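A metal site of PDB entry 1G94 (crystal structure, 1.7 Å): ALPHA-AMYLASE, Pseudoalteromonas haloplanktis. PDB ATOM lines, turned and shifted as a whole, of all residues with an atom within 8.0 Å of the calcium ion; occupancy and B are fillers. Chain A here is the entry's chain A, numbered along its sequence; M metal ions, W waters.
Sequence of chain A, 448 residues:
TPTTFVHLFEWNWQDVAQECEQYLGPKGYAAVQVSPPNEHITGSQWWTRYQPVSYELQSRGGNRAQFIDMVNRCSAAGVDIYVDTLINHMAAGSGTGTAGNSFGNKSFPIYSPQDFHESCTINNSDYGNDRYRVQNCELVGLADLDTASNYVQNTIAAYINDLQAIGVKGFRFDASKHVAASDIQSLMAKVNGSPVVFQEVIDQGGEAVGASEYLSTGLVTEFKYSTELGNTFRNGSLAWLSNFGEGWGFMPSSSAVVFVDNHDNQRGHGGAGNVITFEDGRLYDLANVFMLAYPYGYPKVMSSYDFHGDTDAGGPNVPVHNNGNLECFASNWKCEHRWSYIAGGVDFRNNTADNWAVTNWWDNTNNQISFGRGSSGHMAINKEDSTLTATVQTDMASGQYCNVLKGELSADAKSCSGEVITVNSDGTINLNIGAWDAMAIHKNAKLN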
ATOM      1  N   ILE A  87       7.386  14.889  -1.135  1.00  0.00           N
ATOM      2  CA  ILE A  87       5.988  15.257  -1.350  1.00  0.00           C
ATOM      3  C   ILE A  87       5.132  15.375  -0.088  1.00  0.00           C
ATOM      4  O   ILE A  87       4.003  15.867  -0.142  1.00  0.00           O
ATOM      5  CB  ILE A  87       5.280  14.223  -2.277  1.00  0.00           C
ATOM      6  CG1 ILE A  87       5.254  12.844  -1.616  1.00  0.00           C
ATOM      7  CG2 ILE A  87       5.973  14.166  -3.639  1.00  0.00           C
ATOM      8  CD1 ILE A  87       4.341  11.834  -2.294  1.00  0.00           C
ATOM      9  N   ASN A  88       5.695  14.984   1.059  1.00  0.00           N
ATOM     10  CA  ASN A  88       4.927  14.979   2.309  1.00  0.00           C
ATOM     11  C   ASN A  88       5.088  16.124   3.289  1.00  0.00           C
ATOM     12  O   ASN A  88       4.120  16.505   3.964  1.00  0.00           O
ATOM     13  CB  ASN A  88       5.210  13.657   3.052  1.00  0.00           C
ATOM     14  CG  ASN A  88       4.438  13.536   4.373  1.00  0.00           C
ATOM     15  OD1 ASN A  88       3.214  13.374   4.378  1.00  0.00           O
ATOM     16  ND2 ASN A  88       5.171  13.570   5.491  1.00  0.00           N
ATOM     17  N   HIS A  89       6.270  16.749   3.305  1.00  0.00           N
ATOM     18  CA  HIS A  89       6.525  17.764   4.331  1.00  0.00           C
ATOM     19  C   HIS A  89       7.610  18.798   4.000  1.00  0.00           C
ATOM     20  O   HIS A  89       8.273  18.713   2.961  1.00  0.00           O
ATOM     21  CB  HIS A  89       6.996  17.007   5.588  1.00  0.00           C
ATOM     22  CG  HIS A  89       8.132  16.048   5.312  1.00  0.00           C
ATOM     23  ND1 HIS A  89       7.922  14.700   5.086  1.00  0.00           N
ATOM     24  CD2 HIS A  89       9.460  16.254   5.141  1.00  0.00           C
ATOM     25  CE1 HIS A  89       9.071  14.128   4.763  1.00  0.00           C
ATOM     26  NE2 HIS A  89      10.015  15.046   4.796  1.00  0.00           N
ATOM     27  N   HIS A 117      -1.254  20.750   7.651  1.00  0.00           N
ATOM     28  CA  HIS A 117      -2.259  20.142   8.524  1.00  0.00           C
ATOM     29  C   HIS A 117      -1.971  20.650   9.952  1.00  0.00           C
ATOM     30  O   HIS A 117      -0.847  21.078  10.250  1.00  0.00           O
ATOM     31  CB  HIS A 117      -2.084  18.613   8.521  1.00  0.00           C
ATOM     32  CG  HIS A 117      -2.469  17.951   7.223  1.00  0.00           C
ATOM     33  ND1 HIS A 117      -1.669  16.998   6.621  1.00  0.00           N
ATOM     34  CD2 HIS A 117      -3.582  18.038   6.459  1.00  0.00           C
ATOM     35  CE1 HIS A 117      -2.274  16.536   5.542  1.00  0.00           C
ATOM     36  NE2 HIS A 117      -3.439  17.144   5.421  1.00  0.00           N
ATOM     37  N   ILE A 122       3.014  11.704  15.023  1.00  0.00           N
ATOM     38  CA  ILE A 122       2.767  10.312  14.643  1.00  0.00           C
ATOM     39  C   ILE A 122       3.465   9.443  15.680  1.00  0.00           C
ATOM     40  O   ILE A 122       4.678   9.504  15.842  1.00  0.00           O
ATOM     41  CB  ILE A 122       3.355   9.946  13.268  1.00  0.00           C
ATOM     42  CG1 ILE A 122       2.596  10.652  12.153  1.00  0.00           C
ATOM     43  CG2 ILE A 122       3.248   8.450  13.030  1.00  0.00           C
ATOM     44  CD1 ILE A 122       3.209  10.407  10.782  1.00  0.00           C
ATOM     45  N   TYR A 132      -5.501   7.856   9.800  1.00  0.00           N
ATOM     46  CA  TYR A 132      -5.622   9.305   9.839  1.00  0.00           C
ATOM     47  C   TYR A 132      -4.376   9.978  10.400  1.00  0.00           C
ATOM     48  O   TYR A 132      -3.868  10.924   9.804  1.00  0.00           O
ATOM     49  CB  TYR A 132      -6.847   9.699  10.653  1.00  0.00           C
ATOM     50  CG  TYR A 132      -7.099  11.190  10.697  1.00  0.00           C
ATOM     51  CD1 TYR A 132      -7.837  11.824   9.692  1.00  0.00           C
ATOM     52  CD2 TYR A 132      -6.592  11.970  11.745  1.00  0.00           C
ATOM     53  CE1 TYR A 132      -8.060  13.198   9.739  1.00  0.00           C
ATOM     54  CE2 TYR A 132      -6.812  13.338  11.800  1.00  0.00           C
ATOM     55  CZ  TYR A 132      -7.548  13.950  10.790  1.00  0.00           C
ATOM     56  OH  TYR A 132      -7.794  15.300  10.854  1.00  0.00           O
ATOM     57  N   ARG A 133      -3.858   9.475  11.516  1.00  0.00           N
ATOM     58  CA  ARG A 133      -2.675  10.065  12.144  1.00  0.00           C
ATOM     59  C   ARG A 133      -1.404   9.846  11.328  1.00  0.00           C
ATOM     60  O   ARG A 133      -0.544  10.708  11.259  1.00  0.00           O
ATOM     61  CB  ARG A 133      -2.506   9.547  13.575  1.00  0.00           C
ATOM     62  CG  ARG A 133      -3.586  10.041  14.543  1.00  0.00           C
ATOM     63  CD  ARG A 133      -3.315   9.598  15.966  1.00  0.00           C
ATOM     64  NE  ARG A 133      -2.175  10.286  16.568  1.00  0.00           N
ATOM     65  CZ  ARG A 133      -2.268  11.444  17.220  1.00  0.00           C
ATOM     66  NH1 ARG A 133      -1.168  12.006  17.725  1.00  0.00           N
ATOM     67  NH2 ARG A 133      -3.447  12.013  17.433  1.00  0.00           N
ATOM     68  N   VAL A 134      -1.296   8.677  10.688  1.00  0.00           N
ATOM     69  CA  VAL A 134      -0.134   8.359   9.879  1.00  0.00           C
ATOM     70  C   VAL A 134      -0.046   9.341   8.708  1.00  0.00           C
ATOM     71  O   VAL A 134       1.042   9.779   8.334  1.00  0.00           O
ATOM     72  CB  VAL A 134      -0.217   6.896   9.298  1.00  0.00           C
ATOM     73  CG1 VAL A 134       0.845   6.654   8.215  1.00  0.00           C
ATOM     74  CG2 VAL A 134      -0.029   5.871  10.418  1.00  0.00           C
ATOM     75  N   GLN A 135      -1.212   9.733   8.177  1.00  0.00           N
ATOM     76  CA  GLN A 135      -1.255  10.635   7.023  1.00  0.00           C
ATOM     77  C   GLN A 135      -1.462  12.126   7.262  1.00  0.00           C
ATOM     78  O   GLN A 135      -1.105  12.936   6.394  1.00  0.00           O
ATOM     79  CB  GLN A 135      -2.251  10.072   5.995  1.00  0.00           C
ATOM     80  CG  GLN A 135      -1.812   8.696   5.486  1.00  0.00           C
ATOM     81  CD  GLN A 135      -2.731   8.088   4.445  1.00  0.00           C
ATOM     82  OE1 GLN A 135      -3.912   8.428   4.347  1.00  0.00           O
ATOM     83  NE2 GLN A 135      -2.185   7.163   3.661  1.00  0.00           N
ATOM     84  N   ASN A 136      -1.936  12.500   8.452  1.00  0.00           N
ATOM     85  CA  ASN A 136      -2.187  13.909   8.752  1.00  0.00           C
ATOM     86  C   ASN A 136      -1.302  14.503   9.848  1.00  0.00           C
ATOM     87  O   ASN A 136      -1.184  15.716   9.979  1.00  0.00           O
ATOM     88  CB  ASN A 136      -3.672  14.098   9.096  1.00  0.00           C
ATOM     89  CG  ASN A 136      -4.572  13.796   7.915  1.00  0.00           C
ATOM     90  OD1 ASN A 136      -4.673  14.597   6.984  1.00  0.00           O
ATOM     91  ND2 ASN A 136      -5.196  12.622   7.911  1.00  0.00           N
ATOM     92  N   CYS A 137      -0.656  13.640  10.632  1.00  0.00           N
ATOM     93  CA  CYS A 137       0.234  14.115  11.686  1.00  0.00           C
ATOM     94  C   CYS A 137       1.691  14.188  11.198  1.00  0.00           C
ATOM     95  O   CYS A 137       2.011  13.737  10.090  1.00  0.00           O
ATOM     96  CB  CYS A 137       0.082  13.254  12.951  1.00  0.00           C
ATOM     97  SG  CYS A 137      -1.581  13.398  13.718  1.00  0.00           S
ATOM     98  N   GLU A 138       2.564  14.696  12.059  1.00  0.00           N
ATOM     99  CA  GLU A 138       3.971  14.898  11.719  1.00  0.00           C
ATOM    100  C   GLU A 138       4.909  13.724  11.927  1.00  0.00           C
ATOM    101  O   GLU A 138       4.926  13.095  12.987  1.00  0.00           O
ATOM    102  CB  GLU A 138       4.513  16.111  12.492  1.00  0.00           C
ATOM    103  CG  GLU A 138       3.686  17.373  12.242  1.00  0.00           C
ATOM    104  CD  GLU A 138       4.031  18.558  13.152  1.00  0.00           C
ATOM    105  OE1 GLU A 138       4.594  18.364  14.254  1.00  0.00           O
ATOM    106  OE2 GLU A 138       3.696  19.705  12.761  1.00  0.00           O
ATOM    107  N   LEU A 139       5.698  13.438  10.893  1.00  0.00           N
ATOM    108  CA  LEU A 139       6.708  12.374  10.933  1.00  0.00           C
ATOM    109  C   LEU A 139       7.933  13.044  11.566  1.00  0.00           C
ATOM    110  O   LEU A 139       8.481  14.000  11.003  1.00  0.00           O
ATOM    111  CB  LEU A 139       7.049  11.921   9.494  1.00  0.00           C
ATOM    112  CG  LEU A 139       8.198  10.935   9.286  1.00  0.00           C
ATOM    113  CD1 LEU A 139       7.911   9.629   9.990  1.00  0.00           C
ATOM    114  CD2 LEU A 139       8.418  10.715   7.799  1.00  0.00           C
ATOM    115  N   LEU A 142       8.377  16.927  11.327  1.00  0.00           N
ATOM    116  CA  LEU A 142       8.401  17.579  10.017  1.00  0.00           C
ATOM    117  C   LEU A 142       7.028  18.170   9.672  1.00  0.00           C
ATOM    118  O   LEU A 142       6.009  17.472   9.787  1.00  0.00           O
ATOM    119  CB  LEU A 142       8.839  16.578   8.962  1.00  0.00           C
ATOM    120  CG  LEU A 142      10.229  15.988   9.221  1.00  0.00           C
ATOM    121  CD1 LEU A 142      10.489  14.783   8.319  1.00  0.00           C
ATOM    122  CD2 LEU A 142      11.299  17.034   9.025  1.00  0.00           C
ATOM    123  N   ALA A 143       6.993  19.449   9.263  1.00  0.00           N
ATOM    124  CA  ALA A 143       5.736  20.134   8.933  1.00  0.00           C
ATOM    125  C   ALA A 143       4.983  19.385   7.848  1.00  0.00           C
ATOM    126  O   ALA A 143       5.470  19.252   6.721  1.00  0.00           O
ATOM    127  CB  ALA A 143       6.020  21.578   8.511  1.00  0.00           C
ATOM    128  N   ASP A 144       3.789  18.882   8.186  1.00  0.00           N
ATOM    129  CA  ASP A 144       2.991  18.064   7.278  1.00  0.00           C
ATOM    130  C   ASP A 144       2.118  18.875   6.333  1.00  0.00           C
ATOM    131  O   ASP A 144       1.107  19.452   6.738  1.00  0.00           O
ATOM    132  CB  ASP A 144       2.139  17.079   8.088  1.00  0.00           C
ATOM    133  CG  ASP A 144       1.816  15.813   7.318  1.00  0.00           C
ATOM    134  OD1 ASP A 144       2.746  15.085   6.920  1.00  0.00           O
ATOM    135  OD2 ASP A 144       0.625  15.527   7.118  1.00  0.00           O
ATOM    136  N   LEU A 145       2.481  18.855   5.051  1.00  0.00           N
ATOM    137  CA  LEU A 145       1.743  19.603   4.029  1.00  0.00           C
ATOM    138  C   LEU A 145       0.320  19.109   3.826  1.00  0.00           C
ATOM    139  O   LEU A 145       0.030  17.915   3.952  1.00  0.00           O
ATOM    140  CB  LEU A 145       2.489  19.531   2.700  1.00  0.00           C
ATOM    141  CG  LEU A 145       3.775  20.357   2.525  1.00  0.00           C
ATOM    142  CD1 LEU A 145       4.561  19.893   1.312  1.00  0.00           C
ATOM    143  CD2 LEU A 145       3.430  21.814   2.407  1.00  0.00           C
ATOM    144  N   ASP A 146      -0.591  20.043   3.552  1.00  0.00           N
ATOM    145  CA  ASP A 146      -1.964  19.694   3.270  1.00  0.00           C
ATOM    146  C   ASP A 146      -1.955  19.263   1.782  1.00  0.00           C
ATOM    147  O   ASP A 146      -2.185  20.065   0.877  1.00  0.00           O
ATOM    148  CB  ASP A 146      -2.890  20.887   3.484  1.00  0.00           C
ATOM    149  CG  ASP A 146      -4.350  20.558   3.200  1.00  0.00           C
ATOM    150  OD1 ASP A 146      -4.676  19.426   2.749  1.00  0.00           O
ATOM    151  OD2 ASP A 146      -5.200  21.447   3.411  1.00  0.00           O
ATOM    152  N   THR A 147      -1.660  17.984   1.554  1.00  0.00           N
ATOM    153  CA  THR A 147      -1.565  17.454   0.206  1.00  0.00           C
ATOM    154  C   THR A 147      -2.897  17.336  -0.550  1.00  0.00           C
ATOM    155  O   THR A 147      -2.930  16.888  -1.714  1.00  0.00           O
ATOM    156  CB  THR A 147      -0.801  16.097   0.222  1.00  0.00           C
ATOM    157  OG1 THR A 147      -1.377  15.240   1.221  1.00  0.00           O
ATOM    158  CG2 THR A 147       0.667  16.336   0.526  1.00  0.00           C
ATOM    159  N   ALA A 175       8.479   9.219   1.577  1.00  0.00           N
ATOM    160  CA  ALA A 175       7.412   9.142   2.585  1.00  0.00           C
ATOM    161  C   ALA A 175       5.983   9.049   2.019  1.00  0.00           C
ATOM    162  O   ALA A 175       5.051   9.621   2.589  1.00  0.00           O
ATOM    163  CB  ALA A 175       7.534  10.356   3.541  1.00  0.00           C
ATOM    164  N   SER A 176       5.791   8.293   0.944  1.00  0.00           N
ATOM    165  CA  SER A 176       4.479   8.158   0.325  1.00  0.00           C
ATOM    166  C   SER A 176       3.420   7.581   1.245  1.00  0.00           C
ATOM    167  O   SER A 176       2.229   7.894   1.102  1.00  0.00           O
ATOM    168  CB  SER A 176       4.560   7.315  -0.941  1.00  0.00           C
ATOM    169  OG  SER A 176       5.370   7.975  -1.882  1.00  0.00           O
ATOM    170  N   LYS A 177       3.833   6.706   2.165  1.00  0.00           N
ATOM    171  CA  LYS A 177       2.873   6.142   3.108  1.00  0.00           C
ATOM    172  C   LYS A 177       2.162   7.246   3.886  1.00  0.00           C
ATOM    173  O   LYS A 177       1.001   7.115   4.276  1.00  0.00           O
ATOM    174  CB  LYS A 177       3.568   5.187   4.092  1.00  0.00           C
ATOM    175  CG  LYS A 177       2.588   4.537   5.069  1.00  0.00           C
ATOM    176  CD  LYS A 177       3.040   3.146   5.556  1.00  0.00           C
ATOM    177  CE  LYS A 177       4.044   3.235   6.661  1.00  0.00           C
ATOM    178  NZ  LYS A 177       4.631   1.886   6.981  1.00  0.00           N
ATOM    179  N   HIS A 178       2.856   8.366   4.072  1.00  0.00           N
ATOM    180  CA  HIS A 178       2.324   9.491   4.822  1.00  0.00           C
ATOM    181  C   HIS A 178       1.426  10.447   4.053  1.00  0.00           C
ATOM    182  O   HIS A 178       1.009  11.497   4.577  1.00  0.00           O
ATOM    183  CB  HIS A 178       3.489  10.212   5.493  1.00  0.00           C
ATOM    184  CG  HIS A 178       4.272   9.324   6.414  1.00  0.00           C
ATOM    185  ND1 HIS A 178       3.841   9.014   7.690  1.00  0.00           N
ATOM    186  CD2 HIS A 178       5.383   8.584   6.201  1.00  0.00           C
ATOM    187  CE1 HIS A 178       4.651   8.110   8.216  1.00  0.00           C
ATOM    188  NE2 HIS A 178       5.598   7.833   7.338  1.00  0.00           N
ATOM    189  N   VAL A 179       1.115  10.092   2.807  1.00  0.00           N
ATOM    190  CA  VAL A 179       0.229  10.875   1.950  1.00  0.00           C
ATOM    191  C   VAL A 179      -0.822   9.921   1.411  1.00  0.00           C
ATOM    192  O   VAL A 179      -0.501   8.822   0.927  1.00  0.00           O
ATOM    193  CB  VAL A 179       1.010  11.501   0.742  1.00  0.00           C
ATOM    194  CG1 VAL A 179       0.049  12.249  -0.178  1.00  0.00           C
ATOM    195  CG2 VAL A 179       2.109  12.416   1.245  1.00  0.00           C
ATOM    196  N   ALA A 180      -2.088  10.331   1.494  1.00  0.00           N
ATOM    197  CA  ALA A 180      -3.185   9.504   1.007  1.00  0.00           C
ATOM    198  C   ALA A 180      -2.958   9.178  -0.473  1.00  0.00           C
ATOM    199  O   ALA A 180      -2.542  10.051  -1.248  1.00  0.00           O
ATOM    200  CB  ALA A 180      -4.497  10.213   1.197  1.00  0.00           C
ATOM    201  N   ASP A 183      -4.533  11.532  -2.779  1.00  0.00           N
ATOM    202  CA  ASP A 183      -3.837  12.817  -2.944  1.00  0.00           C
ATOM    203  C   ASP A 183      -2.733  12.644  -3.989  1.00  0.00           C
ATOM    204  O   ASP A 183      -2.470  13.563  -4.761  1.00  0.00           O
ATOM    205  CB  ASP A 183      -3.195  13.301  -1.649  1.00  0.00           C
ATOM    206  CG  ASP A 183      -4.210  13.805  -0.634  1.00  0.00           C
ATOM    207  OD1 ASP A 183      -3.766  14.129   0.508  1.00  0.00           O
ATOM    208  OD2 ASP A 183      -5.412  13.888  -0.938  1.00  0.00           O
HETATM  209 CA    CA M   1       1.123  13.681   5.498  1.00  0.00          CA
HETATM  210  O   HOH W   1       1.771  12.417   7.591  1.00  0.00           O
HETATM  211  O   HOH W   2       1.636  15.725   4.016  1.00  0.00           O
HETATM  212  O   HOH W   3      -0.798  14.121   3.775  1.00  0.00           O
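Four residues have an atom within 4 Å of the calcium ion: Asn 88, Gln 135, Asp 144 and His 178.
The nearest printed residue that does not touch the calcium ion is Asn 136 (4.4 Å).
The backbone carbonyl oxygen of Val 134 lies within hydrogen-bond range of a ring nitrogen (ND1) of His 178.
The backbone carbonyl oxygen (O) of Asn 88 is in hydrogen-bond range of the backbone NH (N) of Leu 145, 3.1 Å away.
A ring nitrogen (ND1) of His 89 lies within hydrogen-bond range of the side-chain amide nitrogen (ND2) of Asn 88 (3.0 Å).
N of His 117 sits at hydrogen-bond distance from O of Asp 144 (2.8 Å).
NE2 of Gln 135 sits at hydrogen-bond distance from O of Lys 177, 3.2 Å away.
The calcium ion is bound by the backbone carbonyl oxygen (O) of His 178 (2.4 Å).
The calcium ion is bound by OD1 of Asn 88, at 2.4 Å.
The calcium ion is bound by OD2 of Asp 144.
O of Gln 135 binds the calcium ion, at 2.5 Å.
Water W1 binds the calcium ion (2.5 Å).
The side-chain carboxylate (OD1) of Asp 144 binds the calcium ion (2.6 Å).
Water W2 is bound to the calcium ion (2.6 Å).
Water W3 is bound to the calcium ion (2.6 Å).
The calcium ion has eight donor atoms within binding distance.
Water W2 lies within hydrogen-bond range of the backbone carbonyl oxygen (O) of Asn 88 (2.6 Å) and the backbone carbonyl oxygen (O) of Leu 145 (2.7 Å).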
